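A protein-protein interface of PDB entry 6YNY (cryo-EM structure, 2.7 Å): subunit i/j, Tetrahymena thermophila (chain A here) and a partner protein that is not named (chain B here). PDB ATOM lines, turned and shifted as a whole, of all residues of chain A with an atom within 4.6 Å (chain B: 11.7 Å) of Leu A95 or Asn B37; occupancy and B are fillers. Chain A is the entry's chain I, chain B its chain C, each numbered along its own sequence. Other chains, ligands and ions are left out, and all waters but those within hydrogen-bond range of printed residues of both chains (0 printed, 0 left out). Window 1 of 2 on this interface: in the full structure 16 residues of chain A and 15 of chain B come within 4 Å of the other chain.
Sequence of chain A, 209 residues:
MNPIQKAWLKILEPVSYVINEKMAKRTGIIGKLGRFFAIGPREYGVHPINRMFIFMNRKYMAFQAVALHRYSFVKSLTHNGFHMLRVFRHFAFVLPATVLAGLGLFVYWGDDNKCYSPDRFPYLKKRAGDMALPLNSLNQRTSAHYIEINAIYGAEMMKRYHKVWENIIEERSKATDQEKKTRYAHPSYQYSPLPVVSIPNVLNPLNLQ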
ATOM      1  N   PHE A  63      31.120 -24.922 -19.397  1.00  0.00           N
ATOM      2  CA  PHE A  63      30.961 -24.008 -18.273  1.00  0.00           C
ATOM      3  C   PHE A  63      31.310 -24.681 -16.953  1.00  0.00           C
ATOM      4  O   PHE A  63      31.903 -24.050 -16.072  1.00  0.00           O
ATOM      5  CB  PHE A  63      29.533 -23.472 -18.244  1.00  0.00           C
ATOM      6  CG  PHE A  63      29.115 -22.941 -16.914  1.00  0.00           C
ATOM      7  CD1 PHE A  63      29.679 -21.795 -16.404  1.00  0.00           C
ATOM      8  CD2 PHE A  63      28.144 -23.584 -16.180  1.00  0.00           C
ATOM      9  CE1 PHE A  63      29.291 -21.310 -15.185  1.00  0.00           C
ATOM     10  CE2 PHE A  63      27.753 -23.099 -14.961  1.00  0.00           C
ATOM     11  CZ  PHE A  63      28.326 -21.961 -14.465  1.00  0.00           C
ATOM     12  N   ALA A  67      33.920 -23.274 -14.100  1.00  0.00           N
ATOM     13  CA  ALA A  67      33.453 -22.988 -12.751  1.00  0.00           C
ATOM     14  C   ALA A  67      34.091 -23.901 -11.716  1.00  0.00           C
ATOM     15  O   ALA A  67      34.307 -23.482 -10.574  1.00  0.00           O
ATOM     16  CB  ALA A  67      31.934 -23.110 -12.699  1.00  0.00           C
ATOM     17  N   ARG A  70      39.102 -23.921 -10.211  1.00  0.00           N
ATOM     18  CA  ARG A  70      39.453 -22.711  -9.488  1.00  0.00           C
ATOM     19  C   ARG A  70      40.628 -22.979  -8.564  1.00  0.00           C
ATOM     20  O   ARG A  70      40.862 -24.112  -8.137  1.00  0.00           O
ATOM     21  CB  ARG A  70      38.272 -22.185  -8.661  1.00  0.00           C
ATOM     22  CG  ARG A  70      37.035 -21.837  -9.458  1.00  0.00           C
ATOM     23  CD  ARG A  70      37.318 -20.780 -10.494  1.00  0.00           C
ATOM     24  NE  ARG A  70      36.128 -20.426 -11.246  1.00  0.00           N
ATOM     25  CZ  ARG A  70      36.146 -19.702 -12.357  1.00  0.00           C
ATOM     26  NH1 ARG A  70      35.017 -19.419 -12.990  1.00  0.00           N
ATOM     27  NH2 ARG A  70      37.300 -19.270 -12.841  1.00  0.00           N
ATOM     28  N   PHE A  93      34.970 -20.867  -3.940  1.00  0.00           N
ATOM     29  CA  PHE A  93      34.134 -22.059  -3.979  1.00  0.00           C
ATOM     30  C   PHE A  93      32.653 -21.739  -4.139  1.00  0.00           C
ATOM     31  O   PHE A  93      31.806 -22.556  -3.767  1.00  0.00           O
ATOM     32  CB  PHE A  93      34.359 -22.901  -2.724  1.00  0.00           C
ATOM     33  CG  PHE A  93      33.941 -24.331  -2.876  1.00  0.00           C
ATOM     34  CD1 PHE A  93      34.658 -25.191  -3.686  1.00  0.00           C
ATOM     35  CD2 PHE A  93      32.834 -24.817  -2.210  1.00  0.00           C
ATOM     36  CE1 PHE A  93      34.278 -26.502  -3.830  1.00  0.00           C
ATOM     37  CE2 PHE A  93      32.451 -26.130  -2.354  1.00  0.00           C
ATOM     38  CZ  PHE A  93      33.174 -26.972  -3.163  1.00  0.00           C
ATOM     39  N   VAL A  94      32.321 -20.577  -4.696  1.00  0.00           N
ATOM     40  CA  VAL A  94      30.922 -20.239  -4.931  1.00  0.00           C
ATOM     41  C   VAL A  94      30.422 -20.868  -6.222  1.00  0.00           C
ATOM     42  O   VAL A  94      29.348 -21.476  -6.258  1.00  0.00           O
ATOM     43  CB  VAL A  94      30.741 -18.712  -4.942  1.00  0.00           C
ATOM     44  CG1 VAL A  94      29.352 -18.348  -5.414  1.00  0.00           C
ATOM     45  CG2 VAL A  94      30.994 -18.159  -3.566  1.00  0.00           C
ATOM     46  N   LEU A  95      31.186 -20.738  -7.297  1.00  0.00           N
ATOM     47  CA  LEU A  95      30.780 -21.320  -8.567  1.00  0.00           C
ATOM     48  C   LEU A  95      30.816 -22.842  -8.522  1.00  0.00           C
ATOM     49  O   LEU A  95      29.892 -23.487  -9.032  1.00  0.00           O
ATOM     50  CB  LEU A  95      31.661 -20.795  -9.696  1.00  0.00           C
ATOM     51  CG  LEU A  95      31.495 -19.314 -10.011  1.00  0.00           C
ATOM     52  CD1 LEU A  95      32.478 -18.920 -11.077  1.00  0.00           C
ATOM     53  CD2 LEU A  95      30.074 -19.006 -10.449  1.00  0.00           C
ATOM     54  N   PRO A  96      31.849 -23.463  -7.945  1.00  0.00           N
ATOM     55  CA  PRO A  96      31.792 -24.925  -7.790  1.00  0.00           C
ATOM     56  C   PRO A  96      30.553 -25.386  -7.046  1.00  0.00           C
ATOM     57  O   PRO A  96      29.863 -26.306  -7.501  1.00  0.00           O
ATOM     58  CB  PRO A  96      33.084 -25.244  -7.028  1.00  0.00           C
ATOM     59  CG  PRO A  96      33.986 -24.123  -7.308  1.00  0.00           C
ATOM     60  CD  PRO A  96      33.146 -22.915  -7.521  1.00  0.00           C
ATOM     61  N   ALA A  97      30.248 -24.761  -5.908  1.00  0.00           N
ATOM     62  CA  ALA A  97      29.044 -25.117  -5.167  1.00  0.00           C
ATOM     63  C   ALA A  97      27.788 -24.846  -5.977  1.00  0.00           C
ATOM     64  O   ALA A  97      26.782 -25.545  -5.817  1.00  0.00           O
ATOM     65  CB  ALA A  97      28.988 -24.345  -3.852  1.00  0.00           C
ATOM     66  N   THR A  98      27.825 -23.838  -6.847  1.00  0.00           N
ATOM     67  CA  THR A  98      26.659 -23.509  -7.654  1.00  0.00           C
ATOM     68  C   THR A  98      26.445 -24.525  -8.765  1.00  0.00           C
ATOM     69  O   THR A  98      25.303 -24.773  -9.166  1.00  0.00           O
ATOM     70  CB  THR A  98      26.813 -22.102  -8.228  1.00  0.00           C
ATOM     71  OG1 THR A  98      26.850 -21.151  -7.158  1.00  0.00           O
ATOM     72  CG2 THR A  98      25.674 -21.772  -9.151  1.00  0.00           C
ATOM     73  N   VAL A  99      27.522 -25.122  -9.269  1.00  0.00           N
ATOM     74  CA  VAL A  99      27.398 -26.133 -10.311  1.00  0.00           C
ATOM     75  C   VAL A  99      26.952 -27.459  -9.717  1.00  0.00           C
ATOM     76  O   VAL A  99      26.118 -28.162 -10.295  1.00  0.00           O
ATOM     77  CB  VAL A  99      28.729 -26.270 -11.068  1.00  0.00           C
ATOM     78  CG1 VAL A  99      28.673 -27.421 -12.042  1.00  0.00           C
ATOM     79  CG2 VAL A  99      29.056 -24.988 -11.786  1.00  0.00           C
ATOM     80  N   ILE B  28      15.681 -22.459  -5.313  1.00  0.00           N
ATOM     81  CA  ILE B  28      15.193 -21.777  -6.507  1.00  0.00           C
ATOM     82  C   ILE B  28      16.193 -20.720  -6.949  1.00  0.00           C
ATOM     83  O   ILE B  28      16.544 -20.623  -8.129  1.00  0.00           O
ATOM     84  CB  ILE B  28      13.807 -21.166  -6.243  1.00  0.00           C
ATOM     85  CG1 ILE B  28      12.773 -22.272  -6.056  1.00  0.00           C
ATOM     86  CG2 ILE B  28      13.411 -20.241  -7.378  1.00  0.00           C
ATOM     87  CD1 ILE B  28      11.435 -21.776  -5.585  1.00  0.00           C
ATOM     88  N   PHE B  29      16.669 -19.913  -6.002  1.00  0.00           N
ATOM     89  CA  PHE B  29      17.675 -18.911  -6.327  1.00  0.00           C
ATOM     90  C   PHE B  29      18.960 -19.557  -6.827  1.00  0.00           C
ATOM     91  O   PHE B  29      19.578 -19.068  -7.778  1.00  0.00           O
ATOM     92  CB  PHE B  29      17.957 -18.042  -5.104  1.00  0.00           C
ATOM     93  CG  PHE B  29      19.328 -17.455  -5.093  1.00  0.00           C
ATOM     94  CD1 PHE B  29      19.621 -16.333  -5.839  1.00  0.00           C
ATOM     95  CD2 PHE B  29      20.331 -18.029  -4.338  1.00  0.00           C
ATOM     96  CE1 PHE B  29      20.882 -15.802  -5.832  1.00  0.00           C
ATOM     97  CE2 PHE B  29      21.593 -17.498  -4.331  1.00  0.00           C
ATOM     98  CZ  PHE B  29      21.869 -16.383  -5.078  1.00  0.00           C
ATOM     99  N   ILE B  30      19.377 -20.656  -6.198  1.00  0.00           N
ATOM    100  CA  ILE B  30      20.626 -21.303  -6.584  1.00  0.00           C
ATOM    101  C   ILE B  30      20.537 -21.822  -8.011  1.00  0.00           C
ATOM    102  O   ILE B  30      21.514 -21.776  -8.766  1.00  0.00           O
ATOM    103  CB  ILE B  30      20.976 -22.422  -5.588  1.00  0.00           C
ATOM    104  CG1 ILE B  30      21.101 -21.845  -4.180  1.00  0.00           C
ATOM    105  CG2 ILE B  30      22.271 -23.100  -5.979  1.00  0.00           C
ATOM    106  CD1 ILE B  30      21.356 -22.866  -3.118  1.00  0.00           C
ATOM    107  N   PHE B  31      19.369 -22.326  -8.404  1.00  0.00           N
ATOM    108  CA  PHE B  31      19.189 -22.776  -9.779  1.00  0.00           C
ATOM    109  C   PHE B  31      19.223 -21.603 -10.749  1.00  0.00           C
ATOM    110  O   PHE B  31      19.734 -21.731 -11.867  1.00  0.00           O
ATOM    111  CB  PHE B  31      17.878 -23.548  -9.916  1.00  0.00           C
ATOM    112  CG  PHE B  31      17.808 -24.787  -9.074  1.00  0.00           C
ATOM    113  CD1 PHE B  31      18.954 -25.469  -8.713  1.00  0.00           C
ATOM    114  CD2 PHE B  31      16.591 -25.271  -8.645  1.00  0.00           C
ATOM    115  CE1 PHE B  31      18.881 -26.601  -7.943  1.00  0.00           C
ATOM    116  CE2 PHE B  31      16.518 -26.406  -7.874  1.00  0.00           C
ATOM    117  CZ  PHE B  31      17.665 -27.070  -7.524  1.00  0.00           C
ATOM    118  N   ILE B  32      18.680 -20.457 -10.344  1.00  0.00           N
ATOM    119  CA  ILE B  32      18.732 -19.273 -11.194  1.00  0.00           C
ATOM    120  C   ILE B  32      20.147 -18.720 -11.248  1.00  0.00           C
ATOM    121  O   ILE B  32      20.616 -18.275 -12.300  1.00  0.00           O
ATOM    122  CB  ILE B  32      17.734 -18.217 -10.695  1.00  0.00           C
ATOM    123  CG1 ILE B  32      16.315 -18.774 -10.739  1.00  0.00           C
ATOM    124  CG2 ILE B  32      17.835 -16.962 -11.530  1.00  0.00           C
ATOM    125  CD1 ILE B  32      15.301 -17.902 -10.079  1.00  0.00           C
ATOM    126  N   TYR B  33      20.851 -18.737 -10.115  1.00  0.00           N
ATOM    127  CA  TYR B  33      22.208 -18.213 -10.080  1.00  0.00           C
ATOM    128  C   TYR B  33      23.140 -19.048 -10.948  1.00  0.00           C
ATOM    129  O   TYR B  33      24.014 -18.503 -11.631  1.00  0.00           O
ATOM    130  CB  TYR B  33      22.701 -18.156  -8.638  1.00  0.00           C
ATOM    131  CG  TYR B  33      23.999 -17.420  -8.456  1.00  0.00           C
ATOM    132  CD1 TYR B  33      24.053 -16.041  -8.552  1.00  0.00           C
ATOM    133  CD2 TYR B  33      25.170 -18.101  -8.175  1.00  0.00           C
ATOM    134  CE1 TYR B  33      25.236 -15.364  -8.384  1.00  0.00           C
ATOM    135  CE2 TYR B  33      26.356 -17.434  -8.005  1.00  0.00           C
ATOM    136  CZ  TYR B  33      26.385 -16.064  -8.110  1.00  0.00           C
ATOM    137  OH  TYR B  33      27.572 -15.398  -7.942  1.00  0.00           O
ATOM    138  N   CYS B  34      22.966 -20.370 -10.940  1.00  0.00           N
ATOM    139  CA  CYS B  34      23.754 -21.217 -11.826  1.00  0.00           C
ATOM    140  C   CYS B  34      23.427 -20.935 -13.283  1.00  0.00           C
ATOM    141  O   CYS B  34      24.327 -20.847 -14.125  1.00  0.00           O
ATOM    142  CB  CYS B  34      23.506 -22.688 -11.508  1.00  0.00           C
ATOM    143  SG  CYS B  34      24.494 -23.827 -12.496  1.00  0.00           S
ATOM    144  N   THR B  35      22.141 -20.795 -13.600  1.00  0.00           N
ATOM    145  CA  THR B  35      21.745 -20.500 -14.969  1.00  0.00           C
ATOM    146  C   THR B  35      22.347 -19.186 -15.444  1.00  0.00           C
ATOM    147  O   THR B  35      22.830 -19.087 -16.576  1.00  0.00           O
ATOM    148  CB  THR B  35      20.223 -20.457 -15.067  1.00  0.00           C
ATOM    149  OG1 THR B  35      19.674 -21.670 -14.540  1.00  0.00           O
ATOM    150  CG2 THR B  35      19.785 -20.298 -16.495  1.00  0.00           C
ATOM    151  N   MET B  36      22.332 -18.164 -14.588  1.00  0.00           N
ATOM    152  CA  MET B  36      22.877 -16.870 -14.971  1.00  0.00           C
ATOM    153  C   MET B  36      24.374 -16.956 -15.236  1.00  0.00           C
ATOM    154  O   MET B  36      24.870 -16.408 -16.225  1.00  0.00           O
ATOM    155  CB  MET B  36      22.578 -15.843 -13.883  1.00  0.00           C
ATOM    156  CG  MET B  36      22.985 -14.432 -14.228  1.00  0.00           C
ATOM    157  SD  MET B  36      24.721 -14.074 -13.924  1.00  0.00           S
ATOM    158  CE  MET B  36      24.722 -14.005 -12.144  1.00  0.00           C
ATOM    159  N   ASN B  37      25.114 -17.636 -14.358  1.00  0.00           N
ATOM    160  CA  ASN B  37      26.551 -17.775 -14.560  1.00  0.00           C
ATOM    161  C   ASN B  37      26.867 -18.617 -15.787  1.00  0.00           C
ATOM    162  O   ASN B  37      27.854 -18.350 -16.481  1.00  0.00           O
ATOM    163  CB  ASN B  37      27.199 -18.379 -13.318  1.00  0.00           C
ATOM    164  CG  ASN B  37      27.398 -17.365 -12.215  1.00  0.00           C
ATOM    165  OD1 ASN B  37      28.407 -16.667 -12.171  1.00  0.00           O
ATOM    166  ND2 ASN B  37      26.435 -17.280 -11.316  1.00  0.00           N
ATOM    167  N   PHE B  38      26.049 -19.630 -16.069  1.00  0.00           N
ATOM    168  CA  PHE B  38      26.263 -20.449 -17.256  1.00  0.00           C
ATOM    169  C   PHE B  38      26.233 -19.602 -18.518  1.00  0.00           C
ATOM    170  O   PHE B  38      27.016 -19.826 -19.446  1.00  0.00           O
ATOM    171  CB  PHE B  38      25.212 -21.556 -17.302  1.00  0.00           C
ATOM    172  CG  PHE B  38      25.008 -22.156 -18.659  1.00  0.00           C
ATOM    173  CD1 PHE B  38      26.067 -22.647 -19.390  1.00  0.00           C
ATOM    174  CD2 PHE B  38      23.740 -22.257 -19.188  1.00  0.00           C
ATOM    175  CE1 PHE B  38      25.865 -23.197 -20.628  1.00  0.00           C
ATOM    176  CE2 PHE B  38      23.538 -22.812 -20.423  1.00  0.00           C
ATOM    177  CZ  PHE B  38      24.601 -23.286 -21.141  1.00  0.00           C
ATOM    178  N   LEU B  39      25.340 -18.617 -18.569  1.00  0.00           N
ATOM    179  CA  LEU B  39      25.251 -17.755 -19.738  1.00  0.00           C
ATOM    180  C   LEU B  39      26.396 -16.752 -19.779  1.00  0.00           C
ATOM    181  O   LEU B  39      26.899 -16.424 -20.859  1.00  0.00           O
ATOM    182  CB  LEU B  39      23.906 -17.034 -19.742  1.00  0.00           C
ATOM    183  CG  LEU B  39      22.687 -17.950 -19.656  1.00  0.00           C
ATOM    184  CD1 LEU B  39      21.410 -17.146 -19.528  1.00  0.00           C
ATOM    185  CD2 LEU B  39      22.618 -18.864 -20.855  1.00  0.00           C
ATOM    186  N   ALA B  40      26.822 -16.261 -18.617  1.00  0.00           N
ATOM    187  CA  ALA B  40      27.887 -15.267 -18.572  1.00  0.00           C
ATOM    188  C   ALA B  40      29.247 -15.894 -18.844  1.00  0.00           C
ATOM    189  O   ALA B  40      29.986 -15.442 -19.726  1.00  0.00           O
ATOM    190  CB  ALA B  40      27.884 -14.567 -17.219  1.00  0.00           C
ATOM    191  N   TRP B  41      29.603 -16.930 -18.086  1.00  0.00           N
ATOM    192  CA  TRP B  41      30.923 -17.532 -18.229  1.00  0.00           C
ATOM    193  C   TRP B  41      31.088 -18.205 -19.585  1.00  0.00           C
ATOM    194  O   TRP B  41      32.150 -18.099 -20.209  1.00  0.00           O
ATOM    195  CB  TRP B  41      31.166 -18.538 -17.110  1.00  0.00           C
ATOM    196  CG  TRP B  41      31.493 -17.916 -15.797  1.00  0.00           C
ATOM    197  CD1 TRP B  41      30.635 -17.680 -14.771  1.00  0.00           C
ATOM    198  CD2 TRP B  41      32.773 -17.450 -15.364  1.00  0.00           C
ATOM    199  NE1 TRP B  41      31.297 -17.095 -13.724  1.00  0.00           N
ATOM    200  CE2 TRP B  41      32.614 -16.942 -14.063  1.00  0.00           C
ATOM    201  CE3 TRP B  41      34.039 -17.412 -15.951  1.00  0.00           C
ATOM    202  CZ2 TRP B  41      33.670 -16.406 -13.340  1.00  0.00           C
ATOM    203  CZ3 TRP B  41      35.082 -16.880 -15.234  1.00  0.00           C
ATOM    204  CH2 TRP B  41      34.894 -16.382 -13.940  1.00  0.00           C
ATOM    205  N   SER B  42      30.055 -18.905 -20.058  1.00  0.00           N
ATOM    206  CA  SER B  42      30.163 -19.572 -21.348  1.00  0.00           C
ATOM    207  C   SER B  42      30.455 -18.576 -22.455  1.00  0.00           C
ATOM    208  O   SER B  42      31.163 -18.898 -23.413  1.00  0.00           O
ATOM    209  CB  SER B  42      28.884 -20.347 -21.658  1.00  0.00           C
ATOM    210  OG  SER B  42      27.782 -19.479 -21.830  1.00  0.00           O
ATOM    211  N   THR B  43      29.929 -17.360 -22.335  1.00  0.00           N
ATOM    212  CA  THR B  43      30.188 -16.342 -23.340  1.00  0.00           C
ATOM    213  C   THR B  43      31.627 -15.854 -23.274  1.00  0.00           C
ATOM    214  O   THR B  43      32.274 -15.664 -24.309  1.00  0.00           O
ATOM    215  CB  THR B  43      29.220 -15.179 -23.149  1.00  0.00           C
ATOM    216  OG1 THR B  43      27.875 -15.662 -23.202  1.00  0.00           O
ATOM    217  CG2 THR B  43      29.427 -14.142 -24.211  1.00  0.00           C
ATOM    218  N   VAL B  44      32.145 -15.651 -22.065  1.00  0.00           N
ATOM    219  CA  VAL B  44      33.507 -15.149 -21.909  1.00  0.00           C
ATOM    220  C   VAL B  44      34.508 -16.155 -22.458  1.00  0.00           C
ATOM    221  O   VAL B  44      35.350 -15.827 -23.301  1.00  0.00           O
ATOM    222  CB  VAL B  44      33.785 -14.831 -20.431  1.00  0.00           C
ATOM    223  CG1 VAL B  44      35.245 -14.505 -20.221  1.00  0.00           C
ATOM    224  CG2 VAL B  44      32.908 -13.691 -19.962  1.00  0.00           C
ATOM    225  N   VAL B  45      34.429 -17.399 -21.985  1.00  0.00           N
ATOM    226  CA  VAL B  45      35.439 -18.390 -22.327  1.00  0.00           C
ATOM    227  C   VAL B  45      35.336 -18.807 -23.787  1.00  0.00           C
ATOM    228  O   VAL B  45      36.350 -19.124 -24.419  1.00  0.00           O
ATOM    229  CB  VAL B  45      35.316 -19.589 -21.376  1.00  0.00           C
ATOM    230  CG1 VAL B  45      36.329 -20.652 -21.723  1.00  0.00           C
ATOM    231  CG2 VAL B  45      35.490 -19.122 -19.950  1.00  0.00           C
ATOM    232  N   GLU B  46      34.128 -18.820 -24.348  1.00  0.00           N
ATOM    233  CA  GLU B  46      33.966 -19.227 -25.739  1.00  0.00           C
ATOM    234  C   GLU B  46      34.429 -18.147 -26.707  1.00  0.00           C
ATOM    235  O   GLU B  46      35.009 -18.458 -27.751  1.00  0.00           O
ATOM    236  CB  GLU B  46      32.510 -19.581 -26.022  1.00  0.00           C
ATOM    237  CG  GLU B  46      32.049 -20.866 -25.373  1.00  0.00           C
ATOM    238  CD  GLU B  46      30.576 -21.138 -25.601  1.00  0.00           C
ATOM    239  OE1 GLU B  46      30.022 -20.619 -26.591  1.00  0.00           O
ATOM    240  OE2 GLU B  46      29.970 -21.865 -24.787  1.00  0.00           O
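Of the 19 printed residues of chain B, 5 touch a printed residue of chain A.
Hydrophobic or aromatic side chains of chain B within 4 Å of the printed part of chain A: Tyr B33, Phe B38 and Trp B41.
Along chain B the printed residues that touch a printed residue of chain A span positions 33 to 41.
Hydrophobic or aromatic side chains of chain A within 4 Å of the printed part of chain B: Phe A63 and Leu A95.
Among the printed residues, 8 pairs touch across the chains.
Among the printed residues, no Asp or Glu carboxylate lies within 4 Å of a Lys or Arg side-chain nitrogen of the other chain.
The side-chain hydroxyl of Thr A98 is in hydrogen-bond range of the backbone carbonyl oxygen of Val A94 (2.7 Å).
O of Tyr B33 sits at hydrogen-bond distance from ND2 of Asn B37, 2.7 Å away.
The side-chain amide oxygen of Asn B37 sits at hydrogen-bond distance from the indole nitrogen of Trp B41, at 3.3 Å.
The backbone carbonyl oxygen (O) of Phe B38 is in hydrogen-bond range of the side-chain hydroxyl (OG) of Ser B42 (2.5 Å).
Among the printed residues, pairs that only touch across the chains: Arg A70 with Trp B41 (3.2 Å), Leu A95 with Asn B37 (3.3 Å), Leu A95 with Trp B41 (3.4 Å), Phe A63 with Asn B37 (3.5 Å), Thr A98 with Tyr B33 (3.6 Å), Phe A63 with Phe B38 (3.6 Å) and Phe A63 with Trp B41 (3.6 Å).
Of the printed residues of chain B, Phe A63 touches Asn B37 (3.5 Å), Phe B38 (3.6 Å) and Trp B41 (3.6 Å).
No residue of chain B comes within 4 Å of Ala A67.
Of the printed residues of chain B, Arg A70 touches Trp B41.
Of the printed residues of chain B, Leu A95 touches Asn B37 (3.3 Å) and Trp B41 (3.4 Å).
No residue of chain B comes within 4 Å of Pro A96.
No residue of chain B comes within 4 Å of Ala A97.
Thr A98 touches two residues of chain B.
No residue of chain B comes within 4 Å of Val A99.
Of the printed residues of chain A, Tyr B33 touches Thr A98.
Printed residues of chain A within 4 Å of Cys B34: Thr A98.
The nearest residue of chain B that does not touch Leu A95 is Tyr B33 (4.7 Å).
O of Thr A98 is in hydrogen-bond range of SG of Cys B34 (3.6 Å).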
